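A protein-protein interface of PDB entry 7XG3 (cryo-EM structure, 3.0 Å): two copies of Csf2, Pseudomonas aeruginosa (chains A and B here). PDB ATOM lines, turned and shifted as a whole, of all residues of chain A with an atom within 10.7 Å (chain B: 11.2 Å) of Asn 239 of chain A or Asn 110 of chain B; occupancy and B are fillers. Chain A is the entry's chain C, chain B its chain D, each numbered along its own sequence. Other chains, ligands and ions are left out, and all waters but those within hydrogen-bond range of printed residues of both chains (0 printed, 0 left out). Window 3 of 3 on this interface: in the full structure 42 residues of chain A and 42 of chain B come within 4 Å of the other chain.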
ATOM      1  N   ARG A 181      19.004  27.643  -3.184  1.00  0.00           N
ATOM      2  CA  ARG A 181      19.419  28.309  -1.963  1.00  0.00           C
ATOM      3  C   ARG A 181      20.762  28.959  -2.248  1.00  0.00           C
ATOM      4  O   ARG A 181      21.678  28.293  -2.740  1.00  0.00           O
ATOM      5  CB  ARG A 181      19.541  27.305  -0.821  1.00  0.00           C
ATOM      6  CG  ARG A 181      19.529  27.899   0.566  1.00  0.00           C
ATOM      7  CD  ARG A 181      19.387  26.792   1.591  1.00  0.00           C
ATOM      8  NE  ARG A 181      20.345  25.719   1.355  1.00  0.00           N
ATOM      9  CZ  ARG A 181      20.313  24.541   1.962  1.00  0.00           C
ATOM     10  NH1 ARG A 181      19.364  24.238   2.832  1.00  0.00           N
ATOM     11  NH2 ARG A 181      21.258  23.645   1.690  1.00  0.00           N
ATOM     12  N   ASP A 210      36.014  29.389   4.419  1.00  0.00           N
ATOM     13  CA  ASP A 210      35.612  28.022   4.753  1.00  0.00           C
ATOM     14  C   ASP A 210      34.841  27.372   3.607  1.00  0.00           C
ATOM     15  O   ASP A 210      35.103  26.216   3.249  1.00  0.00           O
ATOM     16  CB  ASP A 210      34.774  28.022   6.031  1.00  0.00           C
ATOM     17  CG  ASP A 210      34.502  26.621   6.550  1.00  0.00           C
ATOM     18  OD1 ASP A 210      35.279  25.700   6.223  1.00  0.00           O
ATOM     19  OD2 ASP A 210      33.509  26.439   7.283  1.00  0.00           O
ATOM     20  N   ASN A 214      36.174  24.269   1.321  1.00  0.00           N
ATOM     21  CA  ASN A 214      35.331  23.082   1.192  1.00  0.00           C
ATOM     22  C   ASN A 214      35.007  22.779  -0.267  1.00  0.00           C
ATOM     23  O   ASN A 214      35.051  21.618  -0.688  1.00  0.00           O
ATOM     24  CB  ASN A 214      34.048  23.268   2.002  1.00  0.00           C
ATOM     25  CG  ASN A 214      33.449  21.952   2.464  1.00  0.00           C
ATOM     26  OD1 ASN A 214      33.551  20.932   1.783  1.00  0.00           O
ATOM     27  ND2 ASN A 214      32.821  21.970   3.634  1.00  0.00           N
ATOM     28  N   SER A 215      34.708  23.814  -1.062  1.00  0.00           N
ATOM     29  CA  SER A 215      34.363  23.601  -2.464  1.00  0.00           C
ATOM     30  C   SER A 215      35.568  23.148  -3.281  1.00  0.00           C
ATOM     31  O   SER A 215      35.449  22.239  -4.111  1.00  0.00           O
ATOM     32  CB  SER A 215      33.760  24.875  -3.058  1.00  0.00           C
ATOM     33  OG  SER A 215      34.586  25.996  -2.805  1.00  0.00           O
ATOM     34  N   ALA A 217      38.211  21.616  -2.065  1.00  0.00           N
ATOM     35  CA  ALA A 217      38.551  20.275  -1.600  1.00  0.00           C
ATOM     36  C   ALA A 217      37.613  19.228  -2.186  1.00  0.00           C
ATOM     37  O   ALA A 217      38.051  18.132  -2.557  1.00  0.00           O
ATOM     38  CB  ALA A 217      38.522  20.229  -0.073  1.00  0.00           C
ATOM     39  N   ALA A 218      36.320  19.555  -2.291  1.00  0.00           N
ATOM     40  CA  ALA A 218      35.362  18.645  -2.914  1.00  0.00           C
ATOM     41  C   ALA A 218      35.661  18.461  -4.396  1.00  0.00           C
ATOM     42  O   ALA A 218      35.583  17.344  -4.921  1.00  0.00           O
ATOM     43  CB  ALA A 218      33.939  19.164  -2.710  1.00  0.00           C
ATOM     44  N   ALA A 219      36.023  19.548  -5.086  1.00  0.00           N
ATOM     45  CA  ALA A 219      36.361  19.451  -6.504  1.00  0.00           C
ATOM     46  C   ALA A 219      37.673  18.706  -6.727  1.00  0.00           C
ATOM     47  O   ALA A 219      37.832  18.031  -7.751  1.00  0.00           O
ATOM     48  CB  ALA A 219      36.429  20.845  -7.126  1.00  0.00           C
ATOM     49  N   LYS A 221      38.629  16.277  -4.720  1.00  0.00           N
ATOM     50  CA  LYS A 221      38.231  14.894  -4.481  1.00  0.00           C
ATOM     51  C   LYS A 221      37.511  14.317  -5.697  1.00  0.00           C
ATOM     52  O   LYS A 221      37.635  13.122  -5.993  1.00  0.00           O
ATOM     53  CB  LYS A 221      37.350  14.816  -3.231  1.00  0.00           C
ATOM     54  CG  LYS A 221      36.897  13.412  -2.835  1.00  0.00           C
ATOM     55  CD  LYS A 221      38.069  12.437  -2.759  1.00  0.00           C
ATOM     56  CE  LYS A 221      37.594  10.996  -2.880  1.00  0.00           C
ATOM     57  NZ  LYS A 221      38.728  10.031  -2.901  1.00  0.00           N
ATOM     58  N   LYS A 222      36.769  15.159  -6.426  1.00  0.00           N
ATOM     59  CA  LYS A 222      36.081  14.698  -7.631  1.00  0.00           C
ATOM     60  C   LYS A 222      37.060  14.354  -8.748  1.00  0.00           C
ATOM     61  O   LYS A 222      36.734  13.551  -9.631  1.00  0.00           O
ATOM     62  CB  LYS A 222      35.085  15.755  -8.114  1.00  0.00           C
ATOM     63  CG  LYS A 222      33.826  15.886  -7.265  1.00  0.00           C
ATOM     64  CD  LYS A 222      33.132  14.549  -7.041  1.00  0.00           C
ATOM     65  CE  LYS A 222      32.497  14.020  -8.317  1.00  0.00           C
ATOM     66  NZ  LYS A 222      31.844  12.702  -8.097  1.00  0.00           N
ATOM     67  N   ASN A 239      32.849  14.805   5.337  1.00  0.00           N
ATOM     68  CA  ASN A 239      31.866  15.101   4.302  1.00  0.00           C
ATOM     69  C   ASN A 239      30.861  16.140   4.792  1.00  0.00           C
ATOM     70  O   ASN A 239      29.834  15.800   5.379  1.00  0.00           O
ATOM     71  CB  ASN A 239      31.144  13.822   3.869  1.00  0.00           C
ATOM     72  CG  ASN A 239      30.103  14.071   2.789  1.00  0.00           C
ATOM     73  OD1 ASN A 239      30.251  14.970   1.961  1.00  0.00           O
ATOM     74  ND2 ASN A 239      29.042  13.274   2.799  1.00  0.00           N
ATOM     75  N   GLY A 240      31.174  17.414   4.560  1.00  0.00           N
ATOM     76  CA  GLY A 240      30.268  18.499   4.864  1.00  0.00           C
ATOM     77  C   GLY A 240      29.495  18.947   3.638  1.00  0.00           C
ATOM     78  O   GLY A 240      29.615  18.385   2.547  1.00  0.00           O
ATOM     79  N   ARG A 241      28.685  19.986   3.832  1.00  0.00           N
ATOM     80  CA  ARG A 241      27.906  20.546   2.735  1.00  0.00           C
ATOM     81  C   ARG A 241      27.576  22.010   2.984  1.00  0.00           C
ATOM     82  O   ARG A 241      27.217  22.390   4.101  1.00  0.00           O
ATOM     83  CB  ARG A 241      26.620  19.750   2.524  1.00  0.00           C
ATOM     84  CG  ARG A 241      26.008  19.956   1.161  1.00  0.00           C
ATOM     85  CD  ARG A 241      24.829  19.037   0.938  1.00  0.00           C
ATOM     86  NE  ARG A 241      24.374  19.070  -0.446  1.00  0.00           N
ATOM     87  CZ  ARG A 241      23.563  19.992  -0.947  1.00  0.00           C
ATOM     88  NH1 ARG A 241      23.106  20.988  -0.206  1.00  0.00           N
ATOM     89  NH2 ARG A 241      23.199  19.910  -2.221  1.00  0.00           N
ATOM     90  N   GLY A 242      27.692  22.839   1.945  1.00  0.00           N
ATOM     91  CA  GLY A 242      27.420  24.254   2.065  1.00  0.00           C
ATOM     92  C   GLY A 242      25.951  24.587   1.881  1.00  0.00           C
ATOM     93  O   GLY A 242      25.113  23.733   1.599  1.00  0.00           O
ATOM     94  N   LEU A 243      25.646  25.875   2.051  1.00  0.00           N
ATOM     95  CA  LEU A 243      24.275  26.350   1.895  1.00  0.00           C
ATOM     96  C   LEU A 243      23.870  26.467   0.432  1.00  0.00           C
ATOM     97  O   LEU A 243      22.678  26.398   0.115  1.00  0.00           O
ATOM     98  CB  LEU A 243      24.098  27.702   2.581  1.00  0.00           C
ATOM     99  CG  LEU A 243      23.743  27.716   4.063  1.00  0.00           C
ATOM    100  CD1 LEU A 243      23.509  29.139   4.506  1.00  0.00           C
ATOM    101  CD2 LEU A 243      22.518  26.862   4.321  1.00  0.00           C
ATOM    102  N   LYS A 244      24.836  26.669  -0.466  1.00  0.00           N
ATOM    103  CA  LYS A 244      24.522  26.914  -1.867  1.00  0.00           C
ATOM    104  C   LYS A 244      24.003  25.655  -2.542  1.00  0.00           C
ATOM    105  O   LYS A 244      24.770  24.747  -2.875  1.00  0.00           O
ATOM    106  CB  LYS A 244      25.743  27.451  -2.618  1.00  0.00           C
ATOM    107  CG  LYS A 244      25.651  28.933  -2.942  1.00  0.00           C
ATOM    108  CD  LYS A 244      26.843  29.410  -3.753  1.00  0.00           C
ATOM    109  CE  LYS A 244      26.986  28.631  -5.049  1.00  0.00           C
ATOM    110  NZ  LYS A 244      28.245  28.969  -5.766  1.00  0.00           N
ATOM    111  N   ALA A 245      22.691  25.602  -2.738  1.00  0.00           N
ATOM    112  CA  ALA A 245      22.030  24.472  -3.361  1.00  0.00           C
ATOM    113  C   ALA A 245      21.234  24.955  -4.563  1.00  0.00           C
ATOM    114  O   ALA A 245      20.886  26.129  -4.661  1.00  0.00           O
ATOM    115  CB  ALA A 245      21.102  23.744  -2.384  1.00  0.00           C
ATOM    116  N   ASN B 106      18.442  28.007   6.794  1.00  0.00           N
ATOM    117  CA  ASN B 106      19.393  27.060   7.350  1.00  0.00           C
ATOM    118  C   ASN B 106      20.765  27.714   7.418  1.00  0.00           C
ATOM    119  O   ASN B 106      21.040  28.701   6.732  1.00  0.00           O
ATOM    120  CB  ASN B 106      19.456  25.780   6.507  1.00  0.00           C
ATOM    121  CG  ASN B 106      19.906  24.576   7.304  1.00  0.00           C
ATOM    122  OD1 ASN B 106      20.845  24.656   8.095  1.00  0.00           O
ATOM    123  ND2 ASN B 106      19.242  23.448   7.095  1.00  0.00           N
ATOM    124  N   ALA B 107      21.626  27.157   8.270  1.00  0.00           N
ATOM    125  CA  ALA B 107      23.005  27.605   8.372  1.00  0.00           C
ATOM    126  C   ALA B 107      23.999  26.661   7.717  1.00  0.00           C
ATOM    127  O   ALA B 107      25.164  27.034   7.567  1.00  0.00           O
ATOM    128  CB  ALA B 107      23.406  27.798   9.841  1.00  0.00           C
ATOM    129  N   THR B 108      23.586  25.459   7.331  1.00  0.00           N
ATOM    130  CA  THR B 108      24.515  24.508   6.736  1.00  0.00           C
ATOM    131  C   THR B 108      23.748  23.523   5.870  1.00  0.00           C
ATOM    132  O   THR B 108      22.523  23.412   5.946  1.00  0.00           O
ATOM    133  CB  THR B 108      25.318  23.755   7.804  1.00  0.00           C
ATOM    134  OG1 THR B 108      26.038  22.679   7.189  1.00  0.00           O
ATOM    135  CG2 THR B 108      24.396  23.198   8.878  1.00  0.00           C
ATOM    136  N   GLY B 109      24.498  22.806   5.038  1.00  0.00           N
ATOM    137  CA  GLY B 109      24.004  21.573   4.475  1.00  0.00           C
ATOM    138  C   GLY B 109      24.112  20.451   5.485  1.00  0.00           C
ATOM    139  O   GLY B 109      24.625  20.662   6.586  1.00  0.00           O
ATOM    140  N   ASN B 110      23.698  19.254   5.042  1.00  0.00           N
ATOM    141  CA  ASN B 110      23.431  18.092   5.892  1.00  0.00           C
ATOM    142  C   ASN B 110      22.816  18.434   7.255  1.00  0.00           C
ATOM    143  O   ASN B 110      23.486  18.330   8.284  1.00  0.00           O
ATOM    144  CB  ASN B 110      24.652  17.193   6.075  1.00  0.00           C
ATOM    145  CG  ASN B 110      25.946  17.939   6.312  1.00  0.00           C
ATOM    146  OD1 ASN B 110      26.768  18.081   5.409  1.00  0.00           O
ATOM    147  ND2 ASN B 110      26.131  18.430   7.532  1.00  0.00           N
ATOM    148  N   PRO B 111      21.558  18.886   7.284  1.00  0.00           N
ATOM    149  CA  PRO B 111      20.931  19.242   8.563  1.00  0.00           C
ATOM    150  C   PRO B 111      20.669  18.000   9.402  1.00  0.00           C
ATOM    151  O   PRO B 111      20.550  16.896   8.875  1.00  0.00           O
ATOM    152  CB  PRO B 111      19.628  19.917   8.131  1.00  0.00           C
ATOM    153  CG  PRO B 111      19.282  19.232   6.870  1.00  0.00           C
ATOM    154  CD  PRO B 111      20.592  18.973   6.173  1.00  0.00           C
ATOM    155  N   ASP B 112      20.598  18.184  10.718  1.00  0.00           N
ATOM    156  CA  ASP B 112      20.468  17.038  11.608  1.00  0.00           C
ATOM    157  C   ASP B 112      19.076  16.417  11.528  1.00  0.00           C
ATOM    158  O   ASP B 112      18.079  17.100  11.281  1.00  0.00           O
ATOM    159  CB  ASP B 112      20.840  17.434  13.046  1.00  0.00           C
ATOM    160  CG  ASP B 112      20.093  18.668  13.562  1.00  0.00           C
ATOM    161  OD1 ASP B 112      18.857  18.779  13.436  1.00  0.00           O
ATOM    162  OD2 ASP B 112      20.774  19.548  14.128  1.00  0.00           O
ATOM    163  N   GLY B 113      19.025  15.097  11.694  1.00  0.00           N
ATOM    164  CA  GLY B 113      17.772  14.375  11.615  1.00  0.00           C
ATOM    165  C   GLY B 113      16.969  14.343  12.892  1.00  0.00           C
ATOM    166  O   GLY B 113      15.876  13.769  12.906  1.00  0.00           O
ATOM    167  N   VAL B 114      17.486  14.933  13.963  1.00  0.00           N
ATOM    168  CA  VAL B 114      16.789  14.983  15.244  1.00  0.00           C
ATOM    169  C   VAL B 114      15.633  15.972  15.132  1.00  0.00           C
ATOM    170  O   VAL B 114      15.688  16.897  14.309  1.00  0.00           O
ATOM    171  CB  VAL B 114      17.758  15.342  16.385  1.00  0.00           C
ATOM    172  CG1 VAL B 114      18.884  14.324  16.451  1.00  0.00           C
ATOM    173  CG2 VAL B 114      18.331  16.733  16.197  1.00  0.00           C
ATOM    174  N   GLY B 135      13.341  27.474   9.009  1.00  0.00           N
ATOM    175  CA  GLY B 135      14.281  26.475   8.550  1.00  0.00           C
ATOM    176  C   GLY B 135      15.044  25.935   9.733  1.00  0.00           C
ATOM    177  O   GLY B 135      14.464  25.572  10.760  1.00  0.00           O
ATOM    178  N   GLY B 136      16.359  25.888   9.579  1.00  0.00           N
ATOM    179  CA  GLY B 136      17.221  25.434  10.636  1.00  0.00           C
ATOM    180  C   GLY B 136      17.682  24.015  10.396  1.00  0.00           C
ATOM    181  O   GLY B 136      17.259  23.354   9.442  1.00  0.00           O
ATOM    182  N   PRO B 137      18.567  23.518  11.260  1.00  0.00           N
ATOM    183  CA  PRO B 137      19.024  22.129  11.105  1.00  0.00           C
ATOM    184  C   PRO B 137      17.951  21.118  11.462  1.00  0.00           C
ATOM    185  O   PRO B 137      17.940  20.007  10.921  1.00  0.00           O
ATOM    186  CB  PRO B 137      20.238  22.048  12.039  1.00  0.00           C
ATOM    187  CG  PRO B 137      20.156  23.231  12.925  1.00  0.00           C
ATOM    188  CD  PRO B 137      19.101  24.166  12.467  1.00  0.00           C
ATOM    189  N   ARG B 138      16.988  21.560  12.270  1.00  0.00           N
ATOM    190  CA  ARG B 138      15.781  20.743  12.551  1.00  0.00           C
ATOM    191  C   ARG B 138      14.664  21.452  11.778  1.00  0.00           C
ATOM    192  O   ARG B 138      14.412  22.633  12.078  1.00  0.00           O
ATOM    193  CB  ARG B 138      15.517  20.667  14.058  1.00  0.00           C
ATOM    194  CG  ARG B 138      15.588  22.009  14.768  1.00  0.00           C
ATOM    195  CD  ARG B 138      15.683  21.856  16.274  1.00  0.00           C
ATOM    196  NE  ARG B 138      15.932  23.132  16.924  1.00  0.00           N
ATOM    197  CZ  ARG B 138      17.123  23.715  16.989  1.00  0.00           C
ATOM    198  NH1 ARG B 138      18.176  23.126  16.450  1.00  0.00           N
ATOM    199  NH2 ARG B 138      17.256  24.883  17.593  1.00  0.00           N
ATOM    200  N   MET B 139      14.018  20.762  10.831  1.00  0.00           N
ATOM    201  CA  MET B 139      13.005  21.428   9.966  1.00  0.00           C
ATOM    202  C   MET B 139      11.851  21.988  10.805  1.00  0.00           C
ATOM    203  O   MET B 139      11.324  21.256  11.664  1.00  0.00           O
ATOM    204  CB  MET B 139      12.451  20.460   8.917  1.00  0.00           C
ATOM    205  CG  MET B 139      12.873  20.799   7.498  1.00  0.00           C
ATOM    206  SD  MET B 139      14.595  20.391   7.121  1.00  0.00           S
ATOM    207  CE  MET B 139      14.658  20.808   5.380  1.00  0.00           C
ATOM    208  N   ALA B 342      19.056  28.988  15.794  1.00  0.00           N
ATOM    209  CA  ALA B 342      20.187  28.774  14.895  1.00  0.00           C
ATOM    210  C   ALA B 342      21.138  27.635  15.283  1.00  0.00           C
ATOM    211  O   ALA B 342      21.614  26.934  14.382  1.00  0.00           O
ATOM    212  CB  ALA B 342      20.993  30.066  14.786  1.00  0.00           C
ATOM    213  N   GLN B 343      21.463  27.437  16.572  1.00  0.00           N
ATOM    214  CA  GLN B 343      22.345  26.331  16.970  1.00  0.00           C
ATOM    215  C   GLN B 343      21.770  24.955  16.655  1.00  0.00           C
ATOM    216  O   GLN B 343      20.582  24.697  16.859  1.00  0.00           O
ATOM    217  CB  GLN B 343      22.727  26.404  18.457  1.00  0.00           C
ATOM    218  CG  GLN B 343      23.710  27.495  18.989  1.00  0.00           C
ATOM    219  CD  GLN B 343      23.749  28.829  18.271  1.00  0.00           C
ATOM    220  OE1 GLN B 343      22.842  29.646  18.378  1.00  0.00           O
ATOM    221  NE2 GLN B 343      24.834  29.064  17.548  1.00  0.00           N
ATOM    222  N   SER B 344      22.633  24.090  16.126  1.00  0.00           N
ATOM    223  CA  SER B 344      22.275  22.708  15.852  1.00  0.00           C
ATOM    224  C   SER B 344      22.192  21.918  17.146  1.00  0.00           C
ATOM    225  O   SER B 344      23.003  22.108  18.057  1.00  0.00           O
ATOM    226  CB  SER B 344      23.297  22.069  14.908  1.00  0.00           C
ATOM    227  OG  SER B 344      23.085  20.673  14.798  1.00  0.00           O
ATOM    228  N   ALA B 345      21.194  21.036  17.229  1.00  0.00           N
ATOM    229  CA  ALA B 345      21.076  20.162  18.391  1.00  0.00           C
ATOM    230  C   ALA B 345      22.210  19.144  18.433  1.00  0.00           C
ATOM    231  O   ALA B 345      22.686  18.779  19.514  1.00  0.00           O
ATOM    232  CB  ALA B 345      19.721  19.460  18.382  1.00  0.00           C
ATOM    233  N   LYS B 346      22.652  18.677  17.271  1.00  0.00           N
ATOM    234  CA  LYS B 346      23.781  17.757  17.206  1.00  0.00           C
ATOM    235  C   LYS B 346      25.099  18.519  17.276  1.00  0.00           C
ATOM    236  O   LYS B 346      25.813  18.451  18.275  1.00  0.00           O
ATOM    237  CB  LYS B 346      23.729  16.920  15.929  1.00  0.00           C
ATOM    238  CG  LYS B 346      24.948  16.031  15.738  1.00  0.00           C
ATOM    239  CD  LYS B 346      24.789  15.104  14.546  1.00  0.00           C
ATOM    240  CE  LYS B 346      25.854  14.023  14.553  1.00  0.00           C
ATOM    241  NZ  LYS B 346      25.943  13.347  15.876  1.00  0.00           N
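Among the printed residues, merely in contact across the chains: Arg 181 of chain A with Asn 106 of chain B, Asn 239 of chain A with Asn 110 of chain B, Gly 240 of chain A with Asn 110 of chain B, Gly 242 of chain A with Gly 109 of chain B, Leu 243 of chain A with Asn 106 of chain B, Leu 243 of chain A with Ala 107 of chain B and Leu 243 of chain A with Thr 108 of chain B.
No position is printed for both chains.
Of the 10 pairs that touch across the chains among the printed residues, none has its exchanged pair printed and touching as well.
Printed residues of chain B within 4 Å of Arg 181 of chain A: Asn 106 (3.99 Å).
Of chain B, only Asn 110 (3.8 Å) comes within 4 Å of Asn 239 of chain A.
Gly 240 of chain A touches just one residue of chain B: Asn 110.
Of the printed residues of chain B, Arg 241 of chain A touches Thr 108 (3.3 Å), Gly 109 (2.9 Å) and Asn 110 (3.1 Å).
Of the printed residues of chain B, Leu 243 of chain A touches Asn 106, Ala 107 and Thr 108.
Printed residues of chain A within 4 Å of Asn 106 of chain B: Arg 181 (3.99 Å) and Leu 243 (3.4 Å).
Of the printed residues of chain A, Ala 107 of chain B touches Leu 243.
Gly 109 of chain B touches just these residues of chain A: Arg 241 (2.9 Å) and Gly 242 (3.6 Å).
Of the printed residues of chain A, Asn 110 of chain B touches Asn 239, Gly 240 and Arg 241.
Of the 19 printed residues of chain B, 5 touch a printed residue of chain A.
Among the printed residues, 10 pairs touch across the chains.
Among the printed residues, no Asp or Glu carboxylate lies within 4 Å of a Lys or Arg side-chain nitrogen of the other chain.
The backbone carbonyl oxygen (O) of Arg 241 of chain A lies within hydrogen-bond range of the side-chain hydroxyl (OG1) of Thr 108 of chain B.
N of Gly 109 of chain B sits at hydrogen-bond distance from O of Arg 241 of chain A (2.9 Å).
The backbone NH (N) of Arg 241 of chain A sits at hydrogen-bond distance from the side-chain amide oxygen (OD1) of Asn 110 of chain B, 3.1 Å away.
NE of Arg 181 of chain A is in hydrogen-bond range of O of Leu 243 of chain A (2.7 Å).
The backbone NH (N) of Arg 181 of chain A sits at hydrogen-bond distance from the backbone carbonyl oxygen (O) of Ala 245 of chain A (2.8 Å).
The side-chain amide oxygen (OD1) of Asn 106 of chain B lies within hydrogen-bond range of the backbone NH (N) of Thr 108 of chain B (3.0 Å).
ND2 of Asn 106 of chain B is in hydrogen-bond range of O of Gly 136 of chain B (3.1 Å).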
